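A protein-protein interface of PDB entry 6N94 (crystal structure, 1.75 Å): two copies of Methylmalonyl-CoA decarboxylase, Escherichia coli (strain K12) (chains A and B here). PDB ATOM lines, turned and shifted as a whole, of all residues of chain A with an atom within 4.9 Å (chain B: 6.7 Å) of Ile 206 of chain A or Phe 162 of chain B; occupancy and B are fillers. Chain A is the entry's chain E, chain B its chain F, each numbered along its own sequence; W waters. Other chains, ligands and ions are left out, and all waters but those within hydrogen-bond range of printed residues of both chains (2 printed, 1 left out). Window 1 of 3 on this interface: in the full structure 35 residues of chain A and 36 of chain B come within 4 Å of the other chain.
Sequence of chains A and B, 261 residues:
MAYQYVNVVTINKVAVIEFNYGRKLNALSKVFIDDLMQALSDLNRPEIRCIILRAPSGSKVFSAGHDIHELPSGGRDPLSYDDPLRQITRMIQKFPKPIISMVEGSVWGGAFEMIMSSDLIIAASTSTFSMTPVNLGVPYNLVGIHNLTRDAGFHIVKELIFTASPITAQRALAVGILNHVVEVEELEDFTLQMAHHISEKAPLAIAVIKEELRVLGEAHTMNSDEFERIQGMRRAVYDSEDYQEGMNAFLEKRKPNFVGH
N of Ala 202 of chain A sits at hydrogen-bond distance from O of Val 134 of chain B (2.9 Å). The side-chain carboxylate (OD1) of Asp 119 of chain A is in salt-bridge range of the side-chain amino group (NZ) of Lys 158 of chain B (2.8 Å).
The backbone carbonyl oxygen (O) of Glu 159 of chain B lies within hydrogen-bond range of the side-chain hydroxyl (OG1) of Thr 163 of chain B (2.7 Å). The backbone NH (N) of Ser 165 of chain B lies close to the side-chain hydroxyl (OG1) of Thr 163 of chain B, 3.1 Å away. The side-chain carboxylate (OD2) of Asp 119 of chain A lies within salt-bridge range of the side-chain amino group (NZ) of Lys 210 of chain A, at 2.8 Å.
Phe 162 of chain B touches Pro 98 of chain A (CD2 to CG, 3.7 Å). Phe 162 of chain B touches Asp 119 of chain A (CE2 to CB, 3.98 Å). Leu 120 of chain A touches Glu 159 of chain B. Ile 198 of chain A touches Phe 162 of chain B (CG1 to O, 3.8 Å). Ile 198 of chain A touches Thr 163 of chain B. CG of Lys 201 of chain A touches O of Phe 162 of chain B (3.7 Å). Thr 163 of chain B touches Lys 201 of chain A (O to CE, 3.3 Å). Ala 205 of chain A touches Val 138 of chain B. Ile 161 of chain B touches Ile 209 of chain A (CG2 to CD1, 3.9 Å). CB of Lys 210 of chain A touches CZ of Phe 162 of chain B, 3.9 Å away.
Of chain B, only Val 134 and Phe 162 come within 4 Å of Ile 206 of chain A. Printed residues of chain B within 4 Å of Ile 209 of chain A: Ile 161 (3.9 Å). Of the printed residues of chain B, Ala 202 of chain A touches Val 134. The nearest residue of chain B that does not touch Ile 206 of chain A is Ile 161 of chain B (5.6 Å). The nearest printed residue of chain A that does not touch Lys 158 of chain B is Leu 120 of chain A (4.3 Å).
Hydrophobic or aromatic side chains of chain A that line the printed part of chain B: Pro 98, Leu 120, Ile 198, Ala 202, Ala 205, Ile 206 and Ile 209. Among the printed residues, Asp or Glu carboxylates within 4 Å of a Lys or Arg side-chain nitrogen of the other chain: Asp 119 of chain A with Lys 158 of chain B (2.8 Å).
No position is printed for both chains. Of the 15 pairs that touch across the chains among the printed residues, none has its exchanged pair printed and touching as well.
Water W1 bridges the side-chain carboxylate (OD1) of Asp 119 of chain A and the side-chain amino group (NZ) of Lys 158 of chain B. Water W2 lies within hydrogen-bond range of the side-chain amino group of Lys 158 of chain B (2.8 Å) and the backbone carbonyl oxygen of Lys 210 of chain A (3.0 Å).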
ATOM      1  N   PRO A  98      10.083 -21.614  -5.716  1.00  0.00           N
ATOM      2  CA  PRO A  98      10.517 -20.233  -5.873  1.00  0.00           C
ATOM      3  C   PRO A  98       9.840 -19.602  -7.091  1.00  0.00           C
ATOM      4  O   PRO A  98       9.741 -20.262  -8.128  1.00  0.00           O
ATOM      5  CB  PRO A  98      12.028 -20.375  -6.093  1.00  0.00           C
ATOM      6  CG  PRO A  98      12.349 -21.693  -5.502  1.00  0.00           C
ATOM      7  CD  PRO A  98      11.173 -22.568  -5.817  1.00  0.00           C
ATOM      8  N   ASP A 119      10.015 -14.181  -4.756  1.00  0.00           N
ATOM      9  CA  ASP A 119      11.209 -14.655  -4.009  1.00  0.00           C
ATOM     10  C   ASP A 119      12.474 -13.915  -4.461  1.00  0.00           C
ATOM     11  O   ASP A 119      13.331 -13.612  -3.597  1.00  0.00           O
ATOM     12  CB  ASP A 119      11.280 -16.182  -4.063  1.00  0.00           C
ATOM     13  CG  ASP A 119       9.980 -16.791  -3.556  1.00  0.00           C
ATOM     14  OD1 ASP A 119       9.607 -16.461  -2.386  1.00  0.00           O
ATOM     15  OD2 ASP A 119       9.329 -17.543  -4.312  1.00  0.00           O
ATOM     16  N   LEU A 120      12.643 -13.693  -5.777  1.00  0.00           N
ATOM     17  CA  LEU A 120      13.857 -13.045  -6.326  1.00  0.00           C
ATOM     18  C   LEU A 120      13.383 -12.100  -7.416  1.00  0.00           C
ATOM     19  O   LEU A 120      12.324 -12.372  -8.025  1.00  0.00           O
ATOM     20  CB  LEU A 120      14.780 -14.111  -6.934  1.00  0.00           C
ATOM     21  CG  LEU A 120      15.735 -14.869  -6.026  1.00  0.00           C
ATOM     22  CD1 LEU A 120      15.021 -16.080  -5.423  1.00  0.00           C
ATOM     23  CD2 LEU A 120      16.951 -15.337  -6.825  1.00  0.00           C
ATOM     24  N   ILE A 198      18.691 -23.590  -9.515  1.00  0.00           N
ATOM     25  CA  ILE A 198      17.809 -23.813  -8.330  1.00  0.00           C
ATOM     26  C   ILE A 198      17.083 -25.152  -8.517  1.00  0.00           C
ATOM     27  O   ILE A 198      16.924 -25.911  -7.503  1.00  0.00           O
ATOM     28  CB  ILE A 198      16.838 -22.633  -8.180  1.00  0.00           C
ATOM     29  CG1 ILE A 198      17.580 -21.366  -7.790  1.00  0.00           C
ATOM     30  CG2 ILE A 198      15.691 -22.940  -7.244  1.00  0.00           C
ATOM     31  CD1 ILE A 198      16.742 -20.093  -7.855  1.00  0.00           C
ATOM     32  N   LYS A 201      18.298 -28.424  -7.010  1.00  0.00           N
ATOM     33  CA  LYS A 201      18.392 -28.486  -5.532  1.00  0.00           C
ATOM     34  C   LYS A 201      17.177 -29.240  -4.984  1.00  0.00           C
ATOM     35  O   LYS A 201      16.212 -29.485  -5.727  1.00  0.00           O
ATOM     36  CB  LYS A 201      18.530 -27.048  -4.998  1.00  0.00           C
ATOM     37  CG  LYS A 201      19.718 -26.259  -5.563  1.00  0.00           C
ATOM     38  CD  LYS A 201      21.094 -26.952  -5.435  1.00  0.00           C
ATOM     39  CE  LYS A 201      22.237 -26.129  -5.995  1.00  0.00           C
ATOM     40  NZ  LYS A 201      23.544 -26.785  -5.763  1.00  0.00           N
ATOM     41  N   ALA A 202      17.135 -29.445  -3.676  1.00  0.00           N
ATOM     42  CA  ALA A 202      16.111 -30.290  -3.022  1.00  0.00           C
ATOM     43  C   ALA A 202      14.821 -29.501  -2.870  1.00  0.00           C
ATOM     44  O   ALA A 202      14.743 -28.543  -2.085  1.00  0.00           O
ATOM     45  CB  ALA A 202      16.623 -30.792  -1.679  1.00  0.00           C
ATOM     46  N   PRO A 203      13.741 -29.888  -3.598  1.00  0.00           N
ATOM     47  CA  PRO A 203      12.550 -29.044  -3.612  1.00  0.00           C
ATOM     48  C   PRO A 203      11.808 -28.991  -2.281  1.00  0.00           C
ATOM     49  O   PRO A 203      11.153 -28.005  -1.990  1.00  0.00           O
ATOM     50  CB  PRO A 203      11.684 -29.665  -4.709  1.00  0.00           C
ATOM     51  CG  PRO A 203      12.163 -31.123  -4.764  1.00  0.00           C
ATOM     52  CD  PRO A 203      13.661 -31.016  -4.547  1.00  0.00           C
ATOM     53  N   LEU A 204      11.812 -30.090  -1.516  1.00  0.00           N
ATOM     54  CA  LEU A 204      11.082 -30.098  -0.228  1.00  0.00           C
ATOM     55  C   LEU A 204      11.792 -29.196   0.777  1.00  0.00           C
ATOM     56  O   LEU A 204      11.088 -28.587   1.624  1.00  0.00           O
ATOM     57  CB  LEU A 204      10.997 -31.534   0.298  1.00  0.00           C
ATOM     58  CG  LEU A 204      10.332 -32.551  -0.621  1.00  0.00           C
ATOM     59  CD1 LEU A 204      10.394 -33.946   0.000  1.00  0.00           C
ATOM     60  CD2 LEU A 204       8.894 -32.174  -0.937  1.00  0.00           C
ATOM     61  N   ALA A 205      13.117 -29.117   0.708  1.00  0.00           N
ATOM     62  CA  ALA A 205      13.898 -28.229   1.578  1.00  0.00           C
ATOM     63  C   ALA A 205      13.593 -26.788   1.184  1.00  0.00           C
ATOM     64  O   ALA A 205      13.327 -25.940   2.066  1.00  0.00           O
ATOM     65  CB  ALA A 205      15.371 -28.557   1.519  1.00  0.00           C
ATOM     66  N   ILE A 206      13.625 -26.488  -0.122  1.00  0.00           N
ATOM     67  CA  ILE A 206      13.265 -25.131  -0.628  1.00  0.00           C
ATOM     68  C   ILE A 206      11.865 -24.770  -0.129  1.00  0.00           C
ATOM     69  O   ILE A 206      11.704 -23.668   0.399  1.00  0.00           O
ATOM     70  CB  ILE A 206      13.392 -25.078  -2.172  1.00  0.00           C
ATOM     71  CG1 ILE A 206      14.880 -25.135  -2.553  1.00  0.00           C
ATOM     72  CG2 ILE A 206      12.677 -23.869  -2.729  1.00  0.00           C
ATOM     73  CD1 ILE A 206      15.163 -25.386  -4.033  1.00  0.00           C
ATOM     74  N   ALA A 207      10.884 -25.675  -0.258  1.00  0.00           N
ATOM     75  CA  ALA A 207       9.489 -25.336   0.062  1.00  0.00           C
ATOM     76  C   ALA A 207       9.372 -25.020   1.546  1.00  0.00           C
ATOM     77  O   ALA A 207       8.752 -24.023   1.904  1.00  0.00           O
ATOM     78  CB  ALA A 207       8.571 -26.474  -0.342  1.00  0.00           C
ATOM     79  N   VAL A 208       9.990 -25.833   2.417  1.00  0.00           N
ATOM     80  CA  VAL A 208       9.770 -25.590   3.875  1.00  0.00           C
ATOM     81  C   VAL A 208      10.530 -24.315   4.270  1.00  0.00           C
ATOM     82  O   VAL A 208      10.010 -23.533   5.104  1.00  0.00           O
ATOM     83  CB  VAL A 208      10.057 -26.835   4.731  1.00  0.00           C
ATOM     84  CG1 VAL A 208      11.530 -27.163   4.812  1.00  0.00           C
ATOM     85  CG2 VAL A 208       9.479 -26.667   6.143  1.00  0.00           C
ATOM     86  N   ILE A 209      11.711 -24.083   3.724  1.00  0.00           N
ATOM     87  CA  ILE A 209      12.441 -22.832   4.040  1.00  0.00           C
ATOM     88  C   ILE A 209      11.654 -21.619   3.532  1.00  0.00           C
ATOM     89  O   ILE A 209      11.557 -20.609   4.286  1.00  0.00           O
ATOM     90  CB  ILE A 209      13.895 -22.843   3.580  1.00  0.00           C
ATOM     91  CG1 ILE A 209      14.654 -23.930   4.336  1.00  0.00           C
ATOM     92  CG2 ILE A 209      14.546 -21.461   3.750  1.00  0.00           C
ATOM     93  CD1 ILE A 209      16.020 -24.290   3.746  1.00  0.00           C
ATOM     94  N   LYS A 210      11.071 -21.690   2.333  1.00  0.00           N
ATOM     95  CA  LYS A 210      10.241 -20.565   1.842  1.00  0.00           C
ATOM     96  C   LYS A 210       9.099 -20.304   2.827  1.00  0.00           C
ATOM     97  O   LYS A 210       8.804 -19.126   3.141  1.00  0.00           O
ATOM     98  CB  LYS A 210       9.718 -20.847   0.439  1.00  0.00           C
ATOM     99  CG  LYS A 210       8.823 -19.760  -0.092  1.00  0.00           C
ATOM    100  CD  LYS A 210       8.535 -19.864  -1.570  1.00  0.00           C
ATOM    101  CE  LYS A 210       7.321 -19.015  -1.884  1.00  0.00           C
ATOM    102  NZ  LYS A 210       7.122 -18.876  -3.347  1.00  0.00           N
ATOM    103  N   MET B 131      25.233 -20.816   1.875  1.00  0.00           N
ATOM    104  CA  MET B 131      24.242 -21.461   2.756  1.00  0.00           C
ATOM    105  C   MET B 131      23.727 -22.694   2.014  1.00  0.00           C
ATOM    106  O   MET B 131      23.154 -22.538   0.933  1.00  0.00           O
ATOM    107  CB  MET B 131      23.119 -20.467   3.090  1.00  0.00           C
ATOM    108  CG  MET B 131      22.273 -20.889   4.274  1.00  0.00           C
ATOM    109  SD  MET B 131      23.314 -21.172   5.695  1.00  0.00           S
ATOM    110  CE  MET B 131      22.265 -22.270   6.636  1.00  0.00           C
ATOM    111  N   VAL B 134      19.845 -26.855   0.926  1.00  0.00           N
ATOM    112  CA  VAL B 134      19.089 -27.329  -0.269  1.00  0.00           C
ATOM    113  C   VAL B 134      20.008 -28.265  -1.094  1.00  0.00           C
ATOM    114  O   VAL B 134      19.486 -28.972  -1.963  1.00  0.00           O
ATOM    115  CB  VAL B 134      18.488 -26.187  -1.109  1.00  0.00           C
ATOM    116  CG1 VAL B 134      17.599 -25.275  -0.273  1.00  0.00           C
ATOM    117  CG2 VAL B 134      19.526 -25.355  -1.858  1.00  0.00           C
ATOM    118  N   VAL B 138      18.035 -30.819   3.537  1.00  0.00           N
ATOM    119  CA  VAL B 138      17.839 -30.585   5.004  1.00  0.00           C
ATOM    120  C   VAL B 138      16.722 -29.600   5.254  1.00  0.00           C
ATOM    121  O   VAL B 138      16.740 -28.520   4.676  1.00  0.00           O
ATOM    122  CB  VAL B 138      19.129 -30.042   5.642  1.00  0.00           C
ATOM    123  CG1 VAL B 138      18.837 -29.500   7.034  1.00  0.00           C
ATOM    124  CG2 VAL B 138      20.152 -31.148   5.667  1.00  0.00           C
ATOM    125  N   VAL B 157      18.406 -13.056   0.846  1.00  0.00           N
ATOM    126  CA  VAL B 157      18.528 -14.300   1.643  1.00  0.00           C
ATOM    127  C   VAL B 157      17.982 -15.484   0.830  1.00  0.00           C
ATOM    128  O   VAL B 157      18.594 -16.567   0.827  1.00  0.00           O
ATOM    129  CB  VAL B 157      17.829 -14.098   3.002  1.00  0.00           C
ATOM    130  CG1 VAL B 157      17.604 -15.393   3.757  1.00  0.00           C
ATOM    131  CG2 VAL B 157      18.651 -13.105   3.805  1.00  0.00           C
ATOM    132  N   LYS B 158      16.843 -15.318   0.146  1.00  0.00           N
ATOM    133  CA  LYS B 158      16.244 -16.401  -0.636  1.00  0.00           C
ATOM    134  C   LYS B 158      17.154 -16.807  -1.806  1.00  0.00           C
ATOM    135  O   LYS B 158      17.306 -18.011  -2.046  1.00  0.00           O
ATOM    136  CB  LYS B 158      14.831 -16.009  -1.085  1.00  0.00           C
ATOM    137  CG  LYS B 158      13.787 -16.069   0.027  1.00  0.00           C
ATOM    138  CD  LYS B 158      12.562 -15.255  -0.412  1.00  0.00           C
ATOM    139  CE  LYS B 158      11.442 -15.185   0.548  1.00  0.00           C
ATOM    140  NZ  LYS B 158      10.154 -14.856  -0.102  1.00  0.00           N
ATOM    141  N   GLU B 159      17.820 -15.851  -2.468  1.00  0.00           N
ATOM    142  CA  GLU B 159      18.819 -16.205  -3.502  1.00  0.00           C
ATOM    143  C   GLU B 159      19.943 -17.047  -2.869  1.00  0.00           C
ATOM    144  O   GLU B 159      20.280 -18.113  -3.441  1.00  0.00           O
ATOM    145  CB  GLU B 159      19.430 -14.960  -4.155  1.00  0.00           C
ATOM    146  CG  GLU B 159      20.516 -15.319  -5.169  1.00  0.00           C
ATOM    147  CD  GLU B 159      21.211 -14.112  -5.797  1.00  0.00           C
ATOM    148  OE1 GLU B 159      20.753 -12.964  -5.563  1.00  0.00           O
ATOM    149  OE2 GLU B 159      22.260 -14.323  -6.428  1.00  0.00           O
ATOM    150  N   LEU B 160      20.498 -16.629  -1.738  1.00  0.00           N
ATOM    151  CA  LEU B 160      21.604 -17.371  -1.081  1.00  0.00           C
ATOM    152  C   LEU B 160      21.175 -18.809  -0.753  1.00  0.00           C
ATOM    153  O   LEU B 160      21.920 -19.789  -1.058  1.00  0.00           O
ATOM    154  CB  LEU B 160      21.976 -16.667   0.228  1.00  0.00           C
ATOM    155  CG  LEU B 160      22.799 -15.400   0.108  1.00  0.00           C
ATOM    156  CD1 LEU B 160      23.067 -14.862   1.504  1.00  0.00           C
ATOM    157  CD2 LEU B 160      24.120 -15.711  -0.597  1.00  0.00           C
ATOM    158  N   ILE B 161      19.985 -18.959  -0.167  1.00  0.00           N
ATOM    159  CA  ILE B 161      19.520 -20.297   0.298  1.00  0.00           C
ATOM    160  C   ILE B 161      19.067 -21.121  -0.901  1.00  0.00           C
ATOM    161  O   ILE B 161      19.413 -22.333  -0.939  1.00  0.00           O
ATOM    162  CB  ILE B 161      18.420 -20.190   1.370  1.00  0.00           C
ATOM    163  CG1 ILE B 161      18.961 -19.439   2.579  1.00  0.00           C
ATOM    164  CG2 ILE B 161      17.912 -21.579   1.728  1.00  0.00           C
ATOM    165  CD1 ILE B 161      17.928 -19.172   3.640  1.00  0.00           C
ATOM    166  N   PHE B 162      18.293 -20.554  -1.829  1.00  0.00           N
ATOM    167  CA  PHE B 162      17.698 -21.368  -2.922  1.00  0.00           C
ATOM    168  C   PHE B 162      18.761 -21.766  -3.956  1.00  0.00           C
ATOM    169  O   PHE B 162      18.654 -22.850  -4.496  1.00  0.00           O
ATOM    170  CB  PHE B 162      16.522 -20.666  -3.595  1.00  0.00           C
ATOM    171  CG  PHE B 162      15.319 -20.373  -2.732  1.00  0.00           C
ATOM    172  CD1 PHE B 162      15.165 -20.933  -1.467  1.00  0.00           C
ATOM    173  CD2 PHE B 162      14.338 -19.530  -3.196  1.00  0.00           C
ATOM    174  CE1 PHE B 162      14.040 -20.647  -0.701  1.00  0.00           C
ATOM    175  CE2 PHE B 162      13.218 -19.243  -2.423  1.00  0.00           C
ATOM    176  CZ  PHE B 162      13.077 -19.787  -1.181  1.00  0.00           C
ATOM    177  N   THR B 163      19.807 -20.987  -4.165  1.00  0.00           N
ATOM    178  CA  THR B 163      20.893 -21.373  -5.114  1.00  0.00           C
ATOM    179  C   THR B 163      21.992 -22.168  -4.411  1.00  0.00           C
ATOM    180  O   THR B 163      22.689 -22.943  -5.086  1.00  0.00           O
ATOM    181  CB  THR B 163      21.528 -20.150  -5.795  1.00  0.00           C
ATOM    182  OG1 THR B 163      22.257 -19.364  -4.847  1.00  0.00           O
ATOM    183  CG2 THR B 163      20.525 -19.248  -6.493  1.00  0.00           C
ATOM    184  N   ALA B 164      22.198 -21.971  -3.120  1.00  0.00           N
ATOM    185  CA  ALA B 164      23.371 -22.475  -2.375  1.00  0.00           C
ATOM    186  C   ALA B 164      24.665 -22.051  -3.083  1.00  0.00           C
ATOM    187  O   ALA B 164      25.706 -22.709  -2.833  1.00  0.00           O
ATOM    188  CB  ALA B 164      23.338 -23.987  -2.252  1.00  0.00           C
ATOM    189  N   SER B 165      24.657 -20.963  -3.851  1.00  0.00           N
ATOM    190  CA  SER B 165      25.874 -20.504  -4.577  1.00  0.00           C
ATOM    191  C   SER B 165      26.693 -19.603  -3.666  1.00  0.00           C
ATOM    192  O   SER B 165      26.130 -18.819  -2.897  1.00  0.00           O
ATOM    193  CB  SER B 165      25.535 -19.762  -5.848  1.00  0.00           C
ATOM    194  OG  SER B 165      24.841 -20.593  -6.733  1.00  0.00           O
HETATM  195  O   HOH W   1       7.445 -15.249  -1.742  1.00  0.00           O
HETATM  196  O   HOH W   2       9.019 -16.443   1.914  1.00  0.00           O
